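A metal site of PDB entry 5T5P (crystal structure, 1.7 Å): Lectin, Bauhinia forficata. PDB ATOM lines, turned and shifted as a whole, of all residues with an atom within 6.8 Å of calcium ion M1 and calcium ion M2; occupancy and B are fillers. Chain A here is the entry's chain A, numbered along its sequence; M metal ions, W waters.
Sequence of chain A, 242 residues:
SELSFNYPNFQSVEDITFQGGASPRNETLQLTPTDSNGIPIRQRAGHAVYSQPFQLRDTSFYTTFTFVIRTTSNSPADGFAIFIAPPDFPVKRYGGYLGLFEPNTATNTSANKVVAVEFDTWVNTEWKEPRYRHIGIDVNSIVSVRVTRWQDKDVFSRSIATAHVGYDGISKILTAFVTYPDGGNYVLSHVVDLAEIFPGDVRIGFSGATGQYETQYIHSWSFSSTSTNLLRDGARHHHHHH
The backbone NH of Glu 118 lies within hydrogen-bond range of the backbone carbonyl oxygen of Gly 136, at 2.8 Å. The side-chain carboxylate (OE1) of Glu 129 sits close to the indole nitrogen (NE1) of Trp 127, 3.1 Å away. The side-chain carboxylate (OE1) of Glu 118 lies close to the side-chain carboxylate (OD2) of Asp 138 (2.5 Å).
The nearest printed residue that does not touch calcium ion M1 is Ser 144 (4.3 Å).
The nearest printed residue that does not touch calcium ion M2 is Val 123 (4.5 Å).
Calcium ion M1 is bound by the side-chain carboxylate (OD2) of Asp 120 (2.2 Å), water W4 (2.3 Å), water W1 (2.3 Å), the side-chain carboxylate (OE2) of Glu 118 (2.3 Å), the side-chain carboxylate (OE1) of Glu 129 (2.3 Å) and a ring nitrogen (NE2) of His 134 (2.4 Å). Calcium ion M1 has six donor atoms within binding distance.
Calcium ion M2 is bound by OD1 of Asn 124, at 2.3 Å. Calcium ion M2 is bound by water W3. O of Trp 122 binds calcium ion M2 (2.4 Å). OE2 of Glu 129 is bound to calcium ion M2, at 2.4 Å. Water W2 binds calcium ion M2, at 2.5 Å. OD2 of Asp 120 is bound to calcium ion M2, 2.5 Å away. OD1 of Asp 120 binds calcium ion M2, at 2.5 Å. Calcium ion M2 has seven donor atoms within binding distance.
Water W1 bridges OE1 of Glu 118 and O of Ile 142.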
ATOM      1  N   ASP A  78     -24.362   8.305   1.187  1.00  0.00           N
ATOM      2  CA  ASP A  78     -23.569   8.358  -0.056  1.00  0.00           C
ATOM      3  C   ASP A  78     -24.181   7.779  -1.255  1.00  0.00           C
ATOM      4  O   ASP A  78     -23.710   7.964  -2.362  1.00  0.00           O
ATOM      5  CB  ASP A  78     -22.179   7.727   0.188  1.00  0.00           C
ATOM      6  CG  ASP A  78     -21.288   8.680   0.917  1.00  0.00           C
ATOM      7  OD1 ASP A  78     -20.656   9.516   0.191  1.00  0.00           O
ATOM      8  OD2 ASP A  78     -21.223   8.704   2.200  1.00  0.00           O
ATOM      9  N   GLY A  95     -18.998   5.655   3.704  1.00  0.00           N
ATOM     10  CA  GLY A  95     -18.783   6.917   2.987  1.00  0.00           C
ATOM     11  C   GLY A  95     -18.769   6.692   1.483  1.00  0.00           C
ATOM     12  O   GLY A  95     -19.506   5.827   0.938  1.00  0.00           O
ATOM     13  N   GLY A  96     -18.033   7.562   0.786  1.00  0.00           N
ATOM     14  CA  GLY A  96     -18.071   7.570  -0.679  1.00  0.00           C
ATOM     15  C   GLY A  96     -17.513   6.346  -1.384  1.00  0.00           C
ATOM     16  O   GLY A  96     -17.788   6.167  -2.551  1.00  0.00           O
ATOM     17  N   TYR A  97     -16.984   5.394  -0.611  1.00  0.00           N
ATOM     18  CA  TYR A  97     -16.507   4.112  -1.104  1.00  0.00           C
ATOM     19  C   TYR A  97     -17.689   3.120  -1.331  1.00  0.00           C
ATOM     20  O   TYR A  97     -17.503   2.116  -1.954  1.00  0.00           O
ATOM     21  CB  TYR A  97     -15.460   3.522  -0.174  1.00  0.00           C
ATOM     22  CG  TYR A  97     -14.294   4.460  -0.001  1.00  0.00           C
ATOM     23  CD1 TYR A  97     -13.378   4.603  -1.024  1.00  0.00           C
ATOM     24  CD2 TYR A  97     -14.162   5.227   1.136  1.00  0.00           C
ATOM     25  CE1 TYR A  97     -12.336   5.530  -0.936  1.00  0.00           C
ATOM     26  CE2 TYR A  97     -13.167   6.203   1.265  1.00  0.00           C
ATOM     27  CZ  TYR A  97     -12.221   6.319   0.252  1.00  0.00           C
ATOM     28  OH  TYR A  97     -11.180   7.253   0.385  1.00  0.00           O
ATOM     29  N   LEU A  98     -18.888   3.530  -0.854  1.00  0.00           N
ATOM     30  CA  LEU A  98     -20.141   2.825  -1.160  1.00  0.00           C
ATOM     31  C   LEU A  98     -20.157   1.414  -0.715  1.00  0.00           C
ATOM     32  O   LEU A  98     -20.968   0.624  -1.188  1.00  0.00           O
ATOM     33  CB  LEU A  98     -20.562   2.917  -2.643  1.00  0.00           C
ATOM     34  CG  LEU A  98     -20.859   4.320  -3.128  1.00  0.00           C
ATOM     35  CD1 LEU A  98     -21.055   4.394  -4.641  1.00  0.00           C
ATOM     36  CD2 LEU A  98     -22.096   4.896  -2.518  1.00  0.00           C
ATOM     37  N   GLU A 118     -23.884   2.264  -9.813  1.00  0.00           N
ATOM     38  CA  GLU A 118     -23.967   3.081  -8.627  1.00  0.00           C
ATOM     39  C   GLU A 118     -24.991   4.188  -8.779  1.00  0.00           C
ATOM     40  O   GLU A 118     -25.142   4.784  -9.891  1.00  0.00           O
ATOM     41  CB  GLU A 118     -22.587   3.594  -8.210  1.00  0.00           C
ATOM     42  CG  GLU A 118     -22.000   4.587  -9.169  1.00  0.00           C
ATOM     43  CD  GLU A 118     -20.814   5.360  -8.586  1.00  0.00           C
ATOM     44  OE1 GLU A 118     -19.859   4.730  -8.074  1.00  0.00           O
ATOM     45  OE2 GLU A 118     -20.822   6.570  -8.729  1.00  0.00           O
ATOM     46  N   ASP A 120     -25.311   7.576  -6.864  1.00  0.00           N
ATOM     47  CA  ASP A 120     -24.341   8.354  -6.056  1.00  0.00           C
ATOM     48  C   ASP A 120     -24.930   9.685  -5.653  1.00  0.00           C
ATOM     49  O   ASP A 120     -25.148  10.580  -6.497  1.00  0.00           O
ATOM     50  CB  ASP A 120     -23.041   8.497  -6.840  1.00  0.00           C
ATOM     51  CG  ASP A 120     -21.937   9.016  -6.015  1.00  0.00           C
ATOM     52  OD1 ASP A 120     -22.212   9.730  -5.004  1.00  0.00           O
ATOM     53  OD2 ASP A 120     -20.724   8.806  -6.313  1.00  0.00           O
ATOM     54  N   THR A 121     -25.244   9.848  -4.351  1.00  0.00           N
ATOM     55  CA  THR A 121     -25.908  10.995  -3.854  1.00  0.00           C
ATOM     56  C   THR A 121     -24.961  12.089  -3.311  1.00  0.00           C
ATOM     57  O   THR A 121     -25.460  13.196  -3.011  1.00  0.00           O
ATOM     58  CB  THR A 121     -26.871  10.710  -2.699  1.00  0.00           C
ATOM     59  OG1 THR A 121     -26.128  10.031  -1.644  1.00  0.00           O
ATOM     60  CG2 THR A 121     -27.940   9.780  -3.119  1.00  0.00           C
ATOM     61  N   TRP A 122     -23.652  11.835  -3.267  1.00  0.00           N
ATOM     62  CA  TRP A 122     -22.735  12.795  -2.675  1.00  0.00           C
ATOM     63  C   TRP A 122     -21.521  13.002  -3.577  1.00  0.00           C
ATOM     64  O   TRP A 122     -20.824  12.068  -3.883  1.00  0.00           O
ATOM     65  CB  TRP A 122     -22.257  12.315  -1.296  1.00  0.00           C
ATOM     66  CG  TRP A 122     -21.214  13.213  -0.693  1.00  0.00           C
ATOM     67  CD1 TRP A 122     -19.869  13.184  -0.955  1.00  0.00           C
ATOM     68  CD2 TRP A 122     -21.408  14.265   0.257  1.00  0.00           C
ATOM     69  NE1 TRP A 122     -19.236  14.192  -0.235  1.00  0.00           N
ATOM     70  CE2 TRP A 122     -20.163  14.859   0.492  1.00  0.00           C
ATOM     71  CE3 TRP A 122     -22.520  14.809   0.845  1.00  0.00           C
ATOM     72  CZ2 TRP A 122     -19.999  15.870   1.402  1.00  0.00           C
ATOM     73  CZ3 TRP A 122     -22.388  15.822   1.717  1.00  0.00           C
ATOM     74  CH2 TRP A 122     -21.134  16.387   1.985  1.00  0.00           C
ATOM     75  N   VAL A 123     -21.337  14.248  -3.993  1.00  0.00           N
ATOM     76  CA  VAL A 123     -20.221  14.568  -4.864  1.00  0.00           C
ATOM     77  C   VAL A 123     -18.909  14.596  -4.042  1.00  0.00           C
ATOM     78  O   VAL A 123     -18.693  15.445  -3.121  1.00  0.00           O
ATOM     79  CB  VAL A 123     -20.442  15.916  -5.551  1.00  0.00           C
ATOM     80  CG1 VAL A 123     -19.178  16.373  -6.295  1.00  0.00           C
ATOM     81  CG2 VAL A 123     -21.696  15.834  -6.456  1.00  0.00           C
ATOM     82  N   ASN A 124     -18.099  13.570  -4.292  1.00  0.00           N
ATOM     83  CA  ASN A 124     -16.834  13.434  -3.625  1.00  0.00           C
ATOM     84  C   ASN A 124     -15.750  14.303  -4.288  1.00  0.00           C
ATOM     85  O   ASN A 124     -15.649  14.324  -5.483  1.00  0.00           O
ATOM     86  CB  ASN A 124     -16.356  12.026  -3.537  1.00  0.00           C
ATOM     87  CG  ASN A 124     -17.169  11.223  -2.501  1.00  0.00           C
ATOM     88  OD1 ASN A 124     -18.191  10.612  -2.848  1.00  0.00           O
ATOM     89  ND2 ASN A 124     -16.766  11.305  -1.249  1.00  0.00           N
ATOM     90  N   TRP A 127     -11.734  11.979  -5.162  1.00  0.00           N
ATOM     91  CA  TRP A 127     -11.412  11.263  -6.399  1.00  0.00           C
ATOM     92  C   TRP A 127     -12.250  11.978  -7.453  1.00  0.00           C
ATOM     93  O   TRP A 127     -13.123  12.812  -7.103  1.00  0.00           O
ATOM     94  CB  TRP A 127     -11.702   9.754  -6.430  1.00  0.00           C
ATOM     95  CG  TRP A 127     -13.036   9.397  -5.974  1.00  0.00           C
ATOM     96  CD1 TRP A 127     -14.217   9.360  -6.708  1.00  0.00           C
ATOM     97  CD2 TRP A 127     -13.372   9.066  -4.650  1.00  0.00           C
ATOM     98  NE1 TRP A 127     -15.258   9.034  -5.847  1.00  0.00           N
ATOM     99  CE2 TRP A 127     -14.754   8.830  -4.593  1.00  0.00           C
ATOM    100  CE3 TRP A 127     -12.611   8.901  -3.476  1.00  0.00           C
ATOM    101  CZ2 TRP A 127     -15.403   8.482  -3.417  1.00  0.00           C
ATOM    102  CZ3 TRP A 127     -13.244   8.571  -2.307  1.00  0.00           C
ATOM    103  CH2 TRP A 127     -14.612   8.288  -2.296  1.00  0.00           C
ATOM    104  N   LYS A 128     -11.963  11.705  -8.709  1.00  0.00           N
ATOM    105  CA  LYS A 128     -12.673  12.343  -9.810  1.00  0.00           C
ATOM    106  C   LYS A 128     -14.100  11.835  -9.938  1.00  0.00           C
ATOM    107  O   LYS A 128     -14.289  10.627 -10.106  1.00  0.00           O
ATOM    108  CB  LYS A 128     -11.939  12.042 -11.165  1.00  0.00           C
ATOM    109  CG  LYS A 128     -12.812  12.323 -12.368  1.00  0.00           C
ATOM    110  CD  LYS A 128     -12.174  12.968 -13.596  1.00  0.00           C
ATOM    111  CE  LYS A 128     -11.220  12.076 -14.378  1.00  0.00           C
ATOM    112  NZ  LYS A 128     -11.413  10.606 -14.232  1.00  0.00           N
ATOM    113  N   GLU A 129     -15.070  12.695  -9.768  1.00  0.00           N
ATOM    114  CA  GLU A 129     -16.388  12.354 -10.186  1.00  0.00           C
ATOM    115  C   GLU A 129     -17.108  13.610 -10.550  1.00  0.00           C
ATOM    116  O   GLU A 129     -16.570  14.714 -10.335  1.00  0.00           O
ATOM    117  CB  GLU A 129     -17.129  11.457  -9.162  1.00  0.00           C
ATOM    118  CG  GLU A 129     -17.246  11.964  -7.787  1.00  0.00           C
ATOM    119  CD  GLU A 129     -18.024  10.940  -6.920  1.00  0.00           C
ATOM    120  OE1 GLU A 129     -17.973   9.758  -7.212  1.00  0.00           O
ATOM    121  OE2 GLU A 129     -18.715  11.373  -5.981  1.00  0.00           O
ATOM    122  N   PRO A 130     -18.259  13.486 -11.218  1.00  0.00           N
ATOM    123  CA  PRO A 130     -18.998  14.697 -11.665  1.00  0.00           C
ATOM    124  C   PRO A 130     -19.405  15.608 -10.543  1.00  0.00           C
ATOM    125  O   PRO A 130     -19.543  15.196  -9.462  1.00  0.00           O
ATOM    126  CB  PRO A 130     -20.265  14.142 -12.326  1.00  0.00           C
ATOM    127  CG  PRO A 130     -20.011  12.721 -12.560  1.00  0.00           C
ATOM    128  CD  PRO A 130     -18.911  12.226 -11.672  1.00  0.00           C
ATOM    129  N   HIS A 134     -25.190  11.576  -9.556  1.00  0.00           N
ATOM    130  CA  HIS A 134     -25.016  10.801 -10.750  1.00  0.00           C
ATOM    131  C   HIS A 134     -25.259   9.323 -10.591  1.00  0.00           C
ATOM    132  O   HIS A 134     -25.213   8.796  -9.490  1.00  0.00           O
ATOM    133  CB  HIS A 134     -23.580  11.027 -11.317  1.00  0.00           C
ATOM    134  CG  HIS A 134     -22.497  10.795 -10.344  1.00  0.00           C
ATOM    135  ND1 HIS A 134     -22.122  11.705  -9.392  1.00  0.00           N
ATOM    136  CD2 HIS A 134     -21.736   9.695 -10.129  1.00  0.00           C
ATOM    137  CE1 HIS A 134     -21.153  11.217  -8.655  1.00  0.00           C
ATOM    138  NE2 HIS A 134     -20.894   9.997  -9.074  1.00  0.00           N
ATOM    139  N   GLY A 136     -23.796   5.718 -12.329  1.00  0.00           N
ATOM    140  CA  GLY A 136     -22.535   5.330 -12.953  1.00  0.00           C
ATOM    141  C   GLY A 136     -22.380   3.832 -13.073  1.00  0.00           C
ATOM    142  O   GLY A 136     -22.965   3.048 -12.328  1.00  0.00           O
ATOM    143  N   ASP A 138     -19.337   1.196 -12.714  1.00  0.00           N
ATOM    144  CA  ASP A 138     -17.996   1.112 -12.104  1.00  0.00           C
ATOM    145  C   ASP A 138     -17.416  -0.223 -12.466  1.00  0.00           C
ATOM    146  O   ASP A 138     -18.048  -1.262 -12.277  1.00  0.00           O
ATOM    147  CB  ASP A 138     -18.052   1.239 -10.570  1.00  0.00           C
ATOM    148  CG  ASP A 138     -18.724   2.476 -10.089  1.00  0.00           C
ATOM    149  OD1 ASP A 138     -18.725   3.486 -10.842  1.00  0.00           O
ATOM    150  OD2 ASP A 138     -19.115   2.512  -8.877  1.00  0.00           O
ATOM    151  N   ILE A 142     -13.753   3.099  -8.018  1.00  0.00           N
ATOM    152  CA  ILE A 142     -14.779   4.089  -7.618  1.00  0.00           C
ATOM    153  C   ILE A 142     -14.912   5.268  -8.591  1.00  0.00           C
ATOM    154  O   ILE A 142     -15.914   5.922  -8.527  1.00  0.00           O
ATOM    155  CB  ILE A 142     -14.509   4.603  -6.201  1.00  0.00           C
ATOM    156  CG1 ILE A 142     -15.729   5.232  -5.535  1.00  0.00           C
ATOM    157  CG2 ILE A 142     -13.353   5.601  -6.125  1.00  0.00           C
ATOM    158  CD1 ILE A 142     -16.912   4.313  -5.262  1.00  0.00           C
ATOM    159  N   VAL A 143     -13.980   5.436  -9.504  1.00  0.00           N
ATOM    160  CA  VAL A 143     -14.119   6.428 -10.581  1.00  0.00           C
ATOM    161  C   VAL A 143     -14.840   5.696 -11.747  1.00  0.00           C
ATOM    162  O   VAL A 143     -14.220   4.877 -12.430  1.00  0.00           O
ATOM    163  CB  VAL A 143     -12.758   6.967 -11.000  1.00  0.00           C
ATOM    164  CG1 VAL A 143     -12.901   7.931 -12.168  1.00  0.00           C
ATOM    165  CG2 VAL A 143     -12.173   7.700  -9.798  1.00  0.00           C
ATOM    166  N   SER A 144     -16.073   6.037 -11.922  1.00  0.00           N
ATOM    167  CA  SER A 144     -16.944   5.396 -12.932  1.00  0.00           C
ATOM    168  C   SER A 144     -16.401   5.461 -14.352  1.00  0.00           C
ATOM    169  O   SER A 144     -15.767   6.477 -14.778  1.00  0.00           O
ATOM    170  CB  SER A 144     -18.317   6.025 -12.907  1.00  0.00           C
ATOM    171  OG  SER A 144     -18.902   5.950 -11.600  1.00  0.00           O
ATOM    172  N   VAL A 147     -20.750   7.596 -16.740  1.00  0.00           N
ATOM    173  CA  VAL A 147     -21.536   8.304 -15.725  1.00  0.00           C
ATOM    174  C   VAL A 147     -22.442   9.301 -16.318  1.00  0.00           C
ATOM    175  O   VAL A 147     -22.078   9.967 -17.322  1.00  0.00           O
ATOM    176  CB  VAL A 147     -20.502   8.861 -14.705  1.00  0.00           C
ATOM    177  CG1 VAL A 147     -19.637   9.997 -15.289  1.00  0.00           C
ATOM    178  CG2 VAL A 147     -21.166   9.264 -13.433  1.00  0.00           C
HETATM  179 CA    CA M   1     -19.526   8.329  -8.083  1.00  0.00          CA
HETATM  180 CA    CA M   2     -19.832   9.983  -4.343  1.00  0.00          CA
HETATM  181  O   HOH W   1     -18.310   6.636  -7.195  1.00  0.00           O
HETATM  182  O   HOH W   2     -18.530   7.905  -4.481  1.00  0.00           O
HETATM  183  O   HOH W   3     -20.944   9.094  -2.483  1.00  0.00           O
HETATM  184  O   HOH W   4     -18.595   8.150 -10.125  1.00  0.00           O
